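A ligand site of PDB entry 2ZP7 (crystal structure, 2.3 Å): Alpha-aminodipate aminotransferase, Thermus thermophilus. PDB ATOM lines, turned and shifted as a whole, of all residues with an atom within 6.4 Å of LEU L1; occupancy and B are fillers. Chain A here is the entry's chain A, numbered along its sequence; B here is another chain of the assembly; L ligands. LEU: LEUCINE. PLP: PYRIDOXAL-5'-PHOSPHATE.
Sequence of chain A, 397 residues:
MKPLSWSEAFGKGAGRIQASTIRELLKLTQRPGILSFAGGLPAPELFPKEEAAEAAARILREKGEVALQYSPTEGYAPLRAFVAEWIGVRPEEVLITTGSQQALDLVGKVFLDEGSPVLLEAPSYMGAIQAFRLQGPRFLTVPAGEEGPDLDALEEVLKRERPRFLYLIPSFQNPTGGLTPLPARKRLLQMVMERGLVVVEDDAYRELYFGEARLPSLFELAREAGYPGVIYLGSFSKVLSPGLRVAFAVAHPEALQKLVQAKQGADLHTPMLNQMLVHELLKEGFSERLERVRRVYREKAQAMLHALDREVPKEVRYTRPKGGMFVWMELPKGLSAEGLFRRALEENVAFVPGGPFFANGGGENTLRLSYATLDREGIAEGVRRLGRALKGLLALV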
ATOM      1  N   THR A  21       8.464  16.628 -10.041  1.00  0.00           N
ATOM      2  CA  THR A  21       8.957  15.544  -9.184  1.00  0.00           C
ATOM      3  C   THR A  21       7.895  15.059  -8.192  1.00  0.00           C
ATOM      4  O   THR A  21       7.781  13.853  -7.963  1.00  0.00           O
ATOM      5  CB  THR A  21      10.252  15.943  -8.417  1.00  0.00           C
ATOM      6  OG1 THR A  21      10.995  16.916  -9.175  1.00  0.00           O
ATOM      7  CG2 THR A  21      11.133  14.708  -8.161  1.00  0.00           C
ATOM      8  N   ILE A  22       7.145  15.983  -7.593  1.00  0.00           N
ATOM      9  CA  ILE A  22       6.059  15.625  -6.675  1.00  0.00           C
ATOM     10  C   ILE A  22       5.019  14.719  -7.366  1.00  0.00           C
ATOM     11  O   ILE A  22       4.801  13.593  -6.920  1.00  0.00           O
ATOM     12  CB  ILE A  22       5.370  16.883  -6.042  1.00  0.00           C
ATOM     13  CG1 ILE A  22       6.154  17.396  -4.825  1.00  0.00           C
ATOM     14  CG2 ILE A  22       3.892  16.585  -5.634  1.00  0.00           C
ATOM     15  CD1 ILE A  22       7.502  18.035  -5.141  1.00  0.00           C
ATOM     16  N   ARG A  23       4.430  15.192  -8.455  1.00  0.00           N
ATOM     17  CA  ARG A  23       3.364  14.445  -9.144  1.00  0.00           C
ATOM     18  C   ARG A  23       3.835  13.118  -9.756  1.00  0.00           C
ATOM     19  O   ARG A  23       3.053  12.169  -9.855  1.00  0.00           O
ATOM     20  CB  ARG A  23       2.633  15.323 -10.179  1.00  0.00           C
ATOM     21  CG  ARG A  23       3.412  15.672 -11.446  1.00  0.00           C
ATOM     22  CD  ARG A  23       2.523  15.498 -12.663  1.00  0.00           C
ATOM     23  NE  ARG A  23       2.531  16.655 -13.560  1.00  0.00           N
ATOM     24  CZ  ARG A  23       1.642  16.852 -14.533  1.00  0.00           C
ATOM     25  NH1 ARG A  23       1.729  17.932 -15.298  1.00  0.00           N
ATOM     26  NH2 ARG A  23       0.662  15.979 -14.734  1.00  0.00           N
ATOM     27  N   LEU A  25       6.411  11.345  -8.488  1.00  0.00           N
ATOM     28  CA  LEU A  25       6.539  10.517  -7.295  1.00  0.00           C
ATOM     29  C   LEU A  25       5.186  10.001  -6.853  1.00  0.00           C
ATOM     30  O   LEU A  25       5.005   8.795  -6.736  1.00  0.00           O
ATOM     31  CB  LEU A  25       7.247  11.244  -6.155  1.00  0.00           C
ATOM     32  CG  LEU A  25       8.766  11.451  -6.255  1.00  0.00           C
ATOM     33  CD1 LEU A  25       9.289  12.083  -4.977  1.00  0.00           C
ATOM     34  CD2 LEU A  25       9.529  10.156  -6.564  1.00  0.00           C
ATOM     35  N   LEU A  26       4.225  10.901  -6.623  1.00  0.00           N
ATOM     36  CA  LEU A  26       2.847  10.536  -6.275  1.00  0.00           C
ATOM     37  C   LEU A  26       2.282   9.308  -7.031  1.00  0.00           C
ATOM     38  O   LEU A  26       1.644   8.442  -6.418  1.00  0.00           O
ATOM     39  CB  LEU A  26       1.917  11.757  -6.406  1.00  0.00           C
ATOM     40  CG  LEU A  26       1.267  12.404  -5.159  1.00  0.00           C
ATOM     41  CD1 LEU A  26       1.877  11.999  -3.806  1.00  0.00           C
ATOM     42  CD2 LEU A  26       1.158  13.932  -5.267  1.00  0.00           C
ATOM     43  N   LEU A  28       3.352   6.461  -7.639  1.00  0.00           N
ATOM     44  CA  LEU A  28       4.346   5.447  -7.220  1.00  0.00           C
ATOM     45  C   LEU A  28       3.742   4.154  -6.670  1.00  0.00           C
ATOM     46  O   LEU A  28       4.373   3.084  -6.765  1.00  0.00           O
ATOM     47  CB  LEU A  28       5.376   6.028  -6.247  1.00  0.00           C
ATOM     48  CG  LEU A  28       5.088   6.258  -4.750  1.00  0.00           C
ATOM     49  CD1 LEU A  28       6.276   6.966  -4.145  1.00  0.00           C
ATOM     50  CD2 LEU A  28       3.804   7.059  -4.485  1.00  0.00           C
ATOM     51  N   ALA A  38      11.194   5.414  -2.823  1.00  0.00           N
ATOM     52  CA  ALA A  38      10.887   6.777  -3.272  1.00  0.00           C
ATOM     53  C   ALA A  38       9.623   7.238  -2.599  1.00  0.00           C
ATOM     54  O   ALA A  38       8.693   6.464  -2.455  1.00  0.00           O
ATOM     55  CB  ALA A  38      10.689   6.790  -4.762  1.00  0.00           C
ATOM     56  N   GLY A  39       9.552   8.478  -2.179  1.00  0.00           N
ATOM     57  CA  GLY A  39       8.329   8.933  -1.514  1.00  0.00           C
ATOM     58  C   GLY A  39       8.200   8.424  -0.083  1.00  0.00           C
ATOM     59  O   GLY A  39       8.207   7.214   0.170  1.00  0.00           O
ATOM     60  N   GLY A  40       8.067   9.360   0.851  1.00  0.00           N
ATOM     61  CA  GLY A  40       7.917   9.024   2.257  1.00  0.00           C
ATOM     62  C   GLY A  40       6.508   8.553   2.570  1.00  0.00           C
ATOM     63  O   GLY A  40       5.826   9.147   3.412  1.00  0.00           O
ATOM     64  N   LEU A  41       6.090   7.478   1.913  1.00  0.00           N
ATOM     65  CA  LEU A  41       4.737   6.944   2.048  1.00  0.00           C
ATOM     66  C   LEU A  41       4.629   6.118   3.333  1.00  0.00           C
ATOM     67  O   LEU A  41       5.270   5.075   3.441  1.00  0.00           O
ATOM     68  CB  LEU A  41       4.345   6.137   0.799  1.00  0.00           C
ATOM     69  CG  LEU A  41       3.490   6.837  -0.269  1.00  0.00           C
ATOM     70  CD1 LEU A  41       4.206   8.016  -0.932  1.00  0.00           C
ATOM     71  CD2 LEU A  41       3.017   5.844  -1.334  1.00  0.00           C
ATOM     72  N   GLN A 101       1.640  20.884   3.191  1.00  0.00           N
ATOM     73  CA  GLN A 101       1.906  21.448   1.881  1.00  0.00           C
ATOM     74  C   GLN A 101       1.134  22.745   1.643  1.00  0.00           C
ATOM     75  O   GLN A 101       1.689  23.708   1.118  1.00  0.00           O
ATOM     76  CB  GLN A 101       1.620  20.434   0.786  1.00  0.00           C
ATOM     77  CG  GLN A 101       1.977  20.921  -0.621  1.00  0.00           C
ATOM     78  CD  GLN A 101       3.444  21.239  -0.742  1.00  0.00           C
ATOM     79  OE1 GLN A 101       3.834  22.355  -1.121  1.00  0.00           O
ATOM     80  NE2 GLN A 101       4.257  20.264  -0.418  1.00  0.00           N
ATOM     81  N   TYR A 125      13.456  20.355   1.707  1.00  0.00           N
ATOM     82  CA  TYR A 125      12.262  19.661   1.281  1.00  0.00           C
ATOM     83  C   TYR A 125      11.708  20.175  -0.065  1.00  0.00           C
ATOM     84  O   TYR A 125      11.450  21.361  -0.237  1.00  0.00           O
ATOM     85  CB  TYR A 125      11.215  19.624   2.416  1.00  0.00           C
ATOM     86  CG  TYR A 125       9.874  19.083   2.002  1.00  0.00           C
ATOM     87  CD1 TYR A 125       9.768  17.871   1.340  1.00  0.00           C
ATOM     88  CD2 TYR A 125       8.709  19.800   2.274  1.00  0.00           C
ATOM     89  CE1 TYR A 125       8.538  17.368   0.941  1.00  0.00           C
ATOM     90  CE2 TYR A 125       7.469  19.316   1.883  1.00  0.00           C
ATOM     91  CZ  TYR A 125       7.393  18.102   1.224  1.00  0.00           C
ATOM     92  OH  TYR A 125       6.165  17.613   0.821  1.00  0.00           O
ATOM     93  N   MET A 126      11.550  19.240  -0.990  1.00  0.00           N
ATOM     94  CA  MET A 126      11.079  19.473  -2.348  1.00  0.00           C
ATOM     95  C   MET A 126       9.726  20.185  -2.425  1.00  0.00           C
ATOM     96  O   MET A 126       9.522  21.068  -3.240  1.00  0.00           O
ATOM     97  CB  MET A 126      10.959  18.118  -3.040  1.00  0.00           C
ATOM     98  CG  MET A 126      11.279  18.096  -4.509  1.00  0.00           C
ATOM     99  SD  MET A 126      11.362  16.355  -5.039  1.00  0.00           S
ATOM    100  CE  MET A 126      10.171  15.580  -3.874  1.00  0.00           C
ATOM    101  N   ASN A 174      13.866  16.359   5.831  1.00  0.00           N
ATOM    102  CA  ASN A 174      13.631  15.798   4.512  1.00  0.00           C
ATOM    103  C   ASN A 174      14.539  16.588   3.563  1.00  0.00           C
ATOM    104  O   ASN A 174      14.355  17.812   3.436  1.00  0.00           O
ATOM    105  CB  ASN A 174      12.148  15.966   4.126  1.00  0.00           C
ATOM    106  CG  ASN A 174      11.726  15.078   2.941  1.00  0.00           C
ATOM    107  OD1 ASN A 174      12.557  14.576   2.217  1.00  0.00           O
ATOM    108  ND2 ASN A 174      10.405  14.897   2.769  1.00  0.00           N
ATOM    109  N   TYR A 205       7.997  15.386  11.078  1.00  0.00           N
ATOM    110  CA  TYR A 205       8.542  14.161  11.653  1.00  0.00           C
ATOM    111  C   TYR A 205       8.693  14.177  13.177  1.00  0.00           C
ATOM    112  O   TYR A 205       9.238  13.233  13.742  1.00  0.00           O
ATOM    113  CB  TYR A 205       9.867  13.835  10.955  1.00  0.00           C
ATOM    114  CG  TYR A 205       9.652  13.682   9.476  1.00  0.00           C
ATOM    115  CD1 TYR A 205       9.161  12.498   8.945  1.00  0.00           C
ATOM    116  CD2 TYR A 205       9.861  14.761   8.628  1.00  0.00           C
ATOM    117  CE1 TYR A 205       8.941  12.357   7.615  1.00  0.00           C
ATOM    118  CE2 TYR A 205       9.625  14.643   7.273  1.00  0.00           C
ATOM    119  CZ  TYR A 205       9.160  13.443   6.772  1.00  0.00           C
ATOM    120  OH  TYR A 205       8.918  13.309   5.434  1.00  0.00           O
ATOM    121  N   LYS A 238       2.350  11.809   8.664  1.00  0.00           N
ATOM    122  CA  LYS A 238       3.360  10.769   8.937  1.00  0.00           C
ATOM    123  C   LYS A 238       3.008   9.990  10.204  1.00  0.00           C
ATOM    124  O   LYS A 238       3.657   9.005  10.561  1.00  0.00           O
ATOM    125  CB  LYS A 238       4.768  11.410   9.056  1.00  0.00           C
ATOM    126  CG  LYS A 238       5.233  12.243   7.830  1.00  0.00           C
ATOM    127  CD  LYS A 238       4.721  11.654   6.503  1.00  0.00           C
ATOM    128  CE  LYS A 238       5.519  12.110   5.275  1.00  0.00           C
ATOM    129  NZ  LYS A 238       5.639  13.672   4.969  1.00  0.00           N
ATOM    130  N   PHE A 326      13.982   8.666   6.293  1.00  0.00           N
ATOM    131  CA  PHE A 326      14.929   8.741   5.173  1.00  0.00           C
ATOM    132  C   PHE A 326      16.366   8.418   5.531  1.00  0.00           C
ATOM    133  O   PHE A 326      16.855   8.773   6.612  1.00  0.00           O
ATOM    134  CB  PHE A 326      14.861  10.113   4.457  1.00  0.00           C
ATOM    135  CG  PHE A 326      13.465  10.560   4.126  1.00  0.00           C
ATOM    136  CD1 PHE A 326      12.715   9.895   3.161  1.00  0.00           C
ATOM    137  CD2 PHE A 326      12.897  11.635   4.785  1.00  0.00           C
ATOM    138  CE1 PHE A 326      11.413  10.305   2.861  1.00  0.00           C
ATOM    139  CE2 PHE A 326      11.595  12.045   4.484  1.00  0.00           C
ATOM    140  CZ  PHE A 326      10.859  11.378   3.517  1.00  0.00           C
ATOM    141  N   VAL A 352      14.513   8.467  -4.982  1.00  0.00           N
ATOM    142  CA  VAL A 352      14.460   9.829  -5.516  1.00  0.00           C
ATOM    143  C   VAL A 352      15.894  10.333  -5.695  1.00  0.00           C
ATOM    144  O   VAL A 352      16.615  10.452  -4.720  1.00  0.00           O
ATOM    145  CB  VAL A 352      13.746  10.844  -4.556  1.00  0.00           C
ATOM    146  CG1 VAL A 352      13.441  12.128  -5.294  1.00  0.00           C
ATOM    147  CG2 VAL A 352      12.474  10.289  -4.005  1.00  0.00           C
ATOM    148  N   PHE A 357      15.941  18.348  -4.491  1.00  0.00           N
ATOM    149  CA  PHE A 357      16.022  18.844  -3.124  1.00  0.00           C
ATOM    150  C   PHE A 357      16.975  20.023  -2.977  1.00  0.00           C
ATOM    151  O   PHE A 357      17.057  20.643  -1.916  1.00  0.00           O
ATOM    152  CB  PHE A 357      16.409  17.711  -2.173  1.00  0.00           C
ATOM    153  CG  PHE A 357      15.431  16.580  -2.157  1.00  0.00           C
ATOM    154  CD1 PHE A 357      14.328  16.600  -1.274  1.00  0.00           C
ATOM    155  CD2 PHE A 357      15.589  15.506  -3.003  1.00  0.00           C
ATOM    156  CE1 PHE A 357      13.417  15.549  -1.245  1.00  0.00           C
ATOM    157  CE2 PHE A 357      14.689  14.450  -2.986  1.00  0.00           C
ATOM    158  CZ  PHE A 357      13.591  14.476  -2.084  1.00  0.00           C
ATOM    159  N   ARG A 368      17.852  10.148  -2.084  1.00  0.00           N
ATOM    160  CA  ARG A 368      17.079   9.901  -0.870  1.00  0.00           C
ATOM    161  C   ARG A 368      16.453   8.516  -0.931  1.00  0.00           C
ATOM    162  O   ARG A 368      15.824   8.162  -1.913  1.00  0.00           O
ATOM    163  CB  ARG A 368      15.997  10.984  -0.665  1.00  0.00           C
ATOM    164  CG  ARG A 368      15.259  10.877   0.648  1.00  0.00           C
ATOM    165  CD  ARG A 368      14.020  11.804   0.671  1.00  0.00           C
ATOM    166  NE  ARG A 368      12.933  11.235  -0.120  1.00  0.00           N
ATOM    167  CZ  ARG A 368      11.727  11.778  -0.237  1.00  0.00           C
ATOM    168  NH1 ARG A 368      11.439  12.905   0.389  1.00  0.00           N
ATOM    169  NH2 ARG A 368      10.817  11.162  -0.983  1.00  0.00           N
ATOM    170  N   SER A 370      13.871   6.022   1.100  1.00  0.00           N
ATOM    171  CA  SER A 370      12.824   5.987   2.126  1.00  0.00           C
ATOM    172  C   SER A 370      12.486   4.528   2.498  1.00  0.00           C
ATOM    173  O   SER A 370      12.241   3.709   1.624  1.00  0.00           O
ATOM    174  CB  SER A 370      11.566   6.732   1.628  1.00  0.00           C
ATOM    175  OG  SER A 370      10.568   6.642   2.615  1.00  0.00           O
ATOM    176  N   TYR B  70      -1.230   8.883   0.499  1.00  0.00           N
ATOM    177  CA  TYR B  70      -0.834   9.779  -0.578  1.00  0.00           C
ATOM    178  C   TYR B  70      -1.277   9.229  -1.924  1.00  0.00           C
ATOM    179  O   TYR B  70      -1.277   8.030  -2.144  1.00  0.00           O
ATOM    180  CB  TYR B  70       0.693   9.974  -0.624  1.00  0.00           C
ATOM    181  CG  TYR B  70       1.226  10.969   0.372  1.00  0.00           C
ATOM    182  CD1 TYR B  70       0.651  12.239   0.479  1.00  0.00           C
ATOM    183  CD2 TYR B  70       2.320  10.664   1.187  1.00  0.00           C
ATOM    184  CE1 TYR B  70       1.143  13.169   1.398  1.00  0.00           C
ATOM    185  CE2 TYR B  70       2.816  11.599   2.124  1.00  0.00           C
ATOM    186  CZ  TYR B  70       2.218  12.836   2.215  1.00  0.00           C
ATOM    187  OH  TYR B  70       2.678  13.764   3.120  1.00  0.00           O
ATOM    188  N   LEU B 268      -0.615  19.118  -2.585  1.00  0.00           N
ATOM    189  CA  LEU B 268      -0.197  17.774  -3.082  1.00  0.00           C
ATOM    190  C   LEU B 268      -1.313  17.079  -3.881  1.00  0.00           C
ATOM    191  O   LEU B 268      -1.138  16.753  -5.063  1.00  0.00           O
ATOM    192  CB  LEU B 268       0.315  16.849  -1.935  1.00  0.00           C
ATOM    193  CG  LEU B 268       1.549  17.268  -1.125  1.00  0.00           C
ATOM    194  CD1 LEU B 268       1.994  16.156  -0.163  1.00  0.00           C
ATOM    195  CD2 LEU B 268       2.712  17.658  -2.083  1.00  0.00           C
HETATM  196  N   LEU L   1       5.839  13.769   1.808  1.00  0.00           N
HETATM  197  CA  LEU L   1       6.198  13.056   0.546  1.00  0.00           C
HETATM  198  C   LEU L   1       7.700  12.798   0.524  1.00  0.00           C
HETATM  199  O   LEU L   1       8.501  13.658   0.860  1.00  0.00           O
HETATM  200  CB  LEU L   1       5.783  13.898  -0.665  1.00  0.00           C
HETATM  201  CG  LEU L   1       5.137  13.286  -1.919  1.00  0.00           C
HETATM  202  CD1 LEU L   1       6.143  12.999  -3.031  1.00  0.00           C
HETATM  203  CD2 LEU L   1       4.141  14.275  -2.437  1.00  0.00           C
HETATM  204  OXT LEU L   1       8.161  11.732   0.159  1.00  0.00           O
HETATM  205  N1  PLP L   2       7.223  18.992   5.435  1.00  0.00           N
HETATM  206  C2  PLP L   2       8.104  17.943   5.367  1.00  0.00           C
HETATM  207  C2A PLP L   2       9.539  18.182   5.729  1.00  0.00           C
HETATM  208  C3  PLP L   2       7.665  16.696   4.960  1.00  0.00           C
HETATM  209  O3  PLP L   2       8.558  15.737   4.550  1.00  0.00           O
HETATM  210  C4  PLP L   2       6.316  16.554   4.622  1.00  0.00           C
HETATM  211  C4A PLP L   2       5.829  15.141   4.331  1.00  0.00           C
HETATM  212  C5  PLP L   2       5.435  17.630   4.704  1.00  0.00           C
HETATM  213  C6  PLP L   2       5.903  18.861   5.119  1.00  0.00           C
HETATM  214  C5A PLP L   2       4.220  17.677   3.793  1.00  0.00           C
HETATM  215  O4P PLP L   2       3.256  16.819   4.379  1.00  0.00           O
HETATM  216  P   PLP L   2       1.706  17.053   4.151  1.00  0.00           P
HETATM  217  O1P PLP L   2       1.310  18.097   3.154  1.00  0.00           O
HETATM  218  O2P PLP L   2       1.055  17.401   5.488  1.00  0.00           O
HETATM  219  O3P PLP L   2       1.197  15.676   3.758  1.00  0.00           O
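NZ of Lys 238 sits close to N of LEU L1 (3.2 Å).
The side-chain hydroxyl (OH) of Tyr 205 sits at hydrogen-bond distance from an oxygen (O3) of PLP L2 (2.6 Å).
O3 of PLP L2 lies within hydrogen-bond range of ND2 of Asn 174 (2.7 Å).
The side-chain amide nitrogen (ND2) of Asn 174 sits at hydrogen-bond distance from an oxygen (O) of LEU L1.
The side-chain hydroxyl of Tyr 70 of chain B sits at hydrogen-bond distance from a nitrogen (N) of LEU L1, 3.4 Å away.
The guanidinium group (NH2) of Arg 368 lies within salt-bridge range of an oxygen (OXT) of LEU L1.
C4A of PLP L2 is bonded to NZ of Lys 238, at 1.6 Å.
The backbone NH (N) of Gly 40 lies within hydrogen-bond range of an oxygen (OXT) of LEU L1, at 2.5 Å.
An oxygen (O1P) of PLP L2 is in hydrogen-bond range of the backbone NH (N) of Gln 101, at 2.8 Å.
OH of Tyr 70 of chain B sits at hydrogen-bond distance from O3P of PLP L2.
Merely in contact with LEU L1: Ile 22, Leu 25, Leu 26, Gly 39, Tyr 125 and Leu 268 of chain B.
11 residues have an atom within 4 Å of LEU L1: Ile 22, Leu 25, Leu 26, Gly 39, Gly 40, Tyr 125, Asn 174, Lys 238, Arg 368, Tyr 70 of chain B and Leu 268 of chain B.
The backbone carbonyl oxygen (O) of Val 352 is in hydrogen-bond range of the backbone NH (N) of Arg 368 (2.9 Å).
The guanidinium group of Arg 368 sits at hydrogen-bond distance from the side-chain amide oxygen of Asn 174 (2.7 Å).
OG of Ser 370 lies within hydrogen-bond range of O of Gly 39 (3.4 Å).
The side-chain hydroxyl (OH) of Tyr 125 sits at hydrogen-bond distance from the side-chain amide nitrogen (NE2) of Gln 101.
O of Asn 174 lies within hydrogen-bond range of N of Tyr 125 (3.2 Å).
The side-chain amino group of Lys 238 is in hydrogen-bond range of the side-chain hydroxyl of Tyr 70 of chain B (3.5 Å).
The side-chain amide nitrogen of Asn 174 is in hydrogen-bond range of the side-chain hydroxyl of Tyr 205, 3.4 Å away.
The side-chain amino group of Lys 238 sits at hydrogen-bond distance from the side-chain hydroxyl of Tyr 205, 3.3 Å away.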
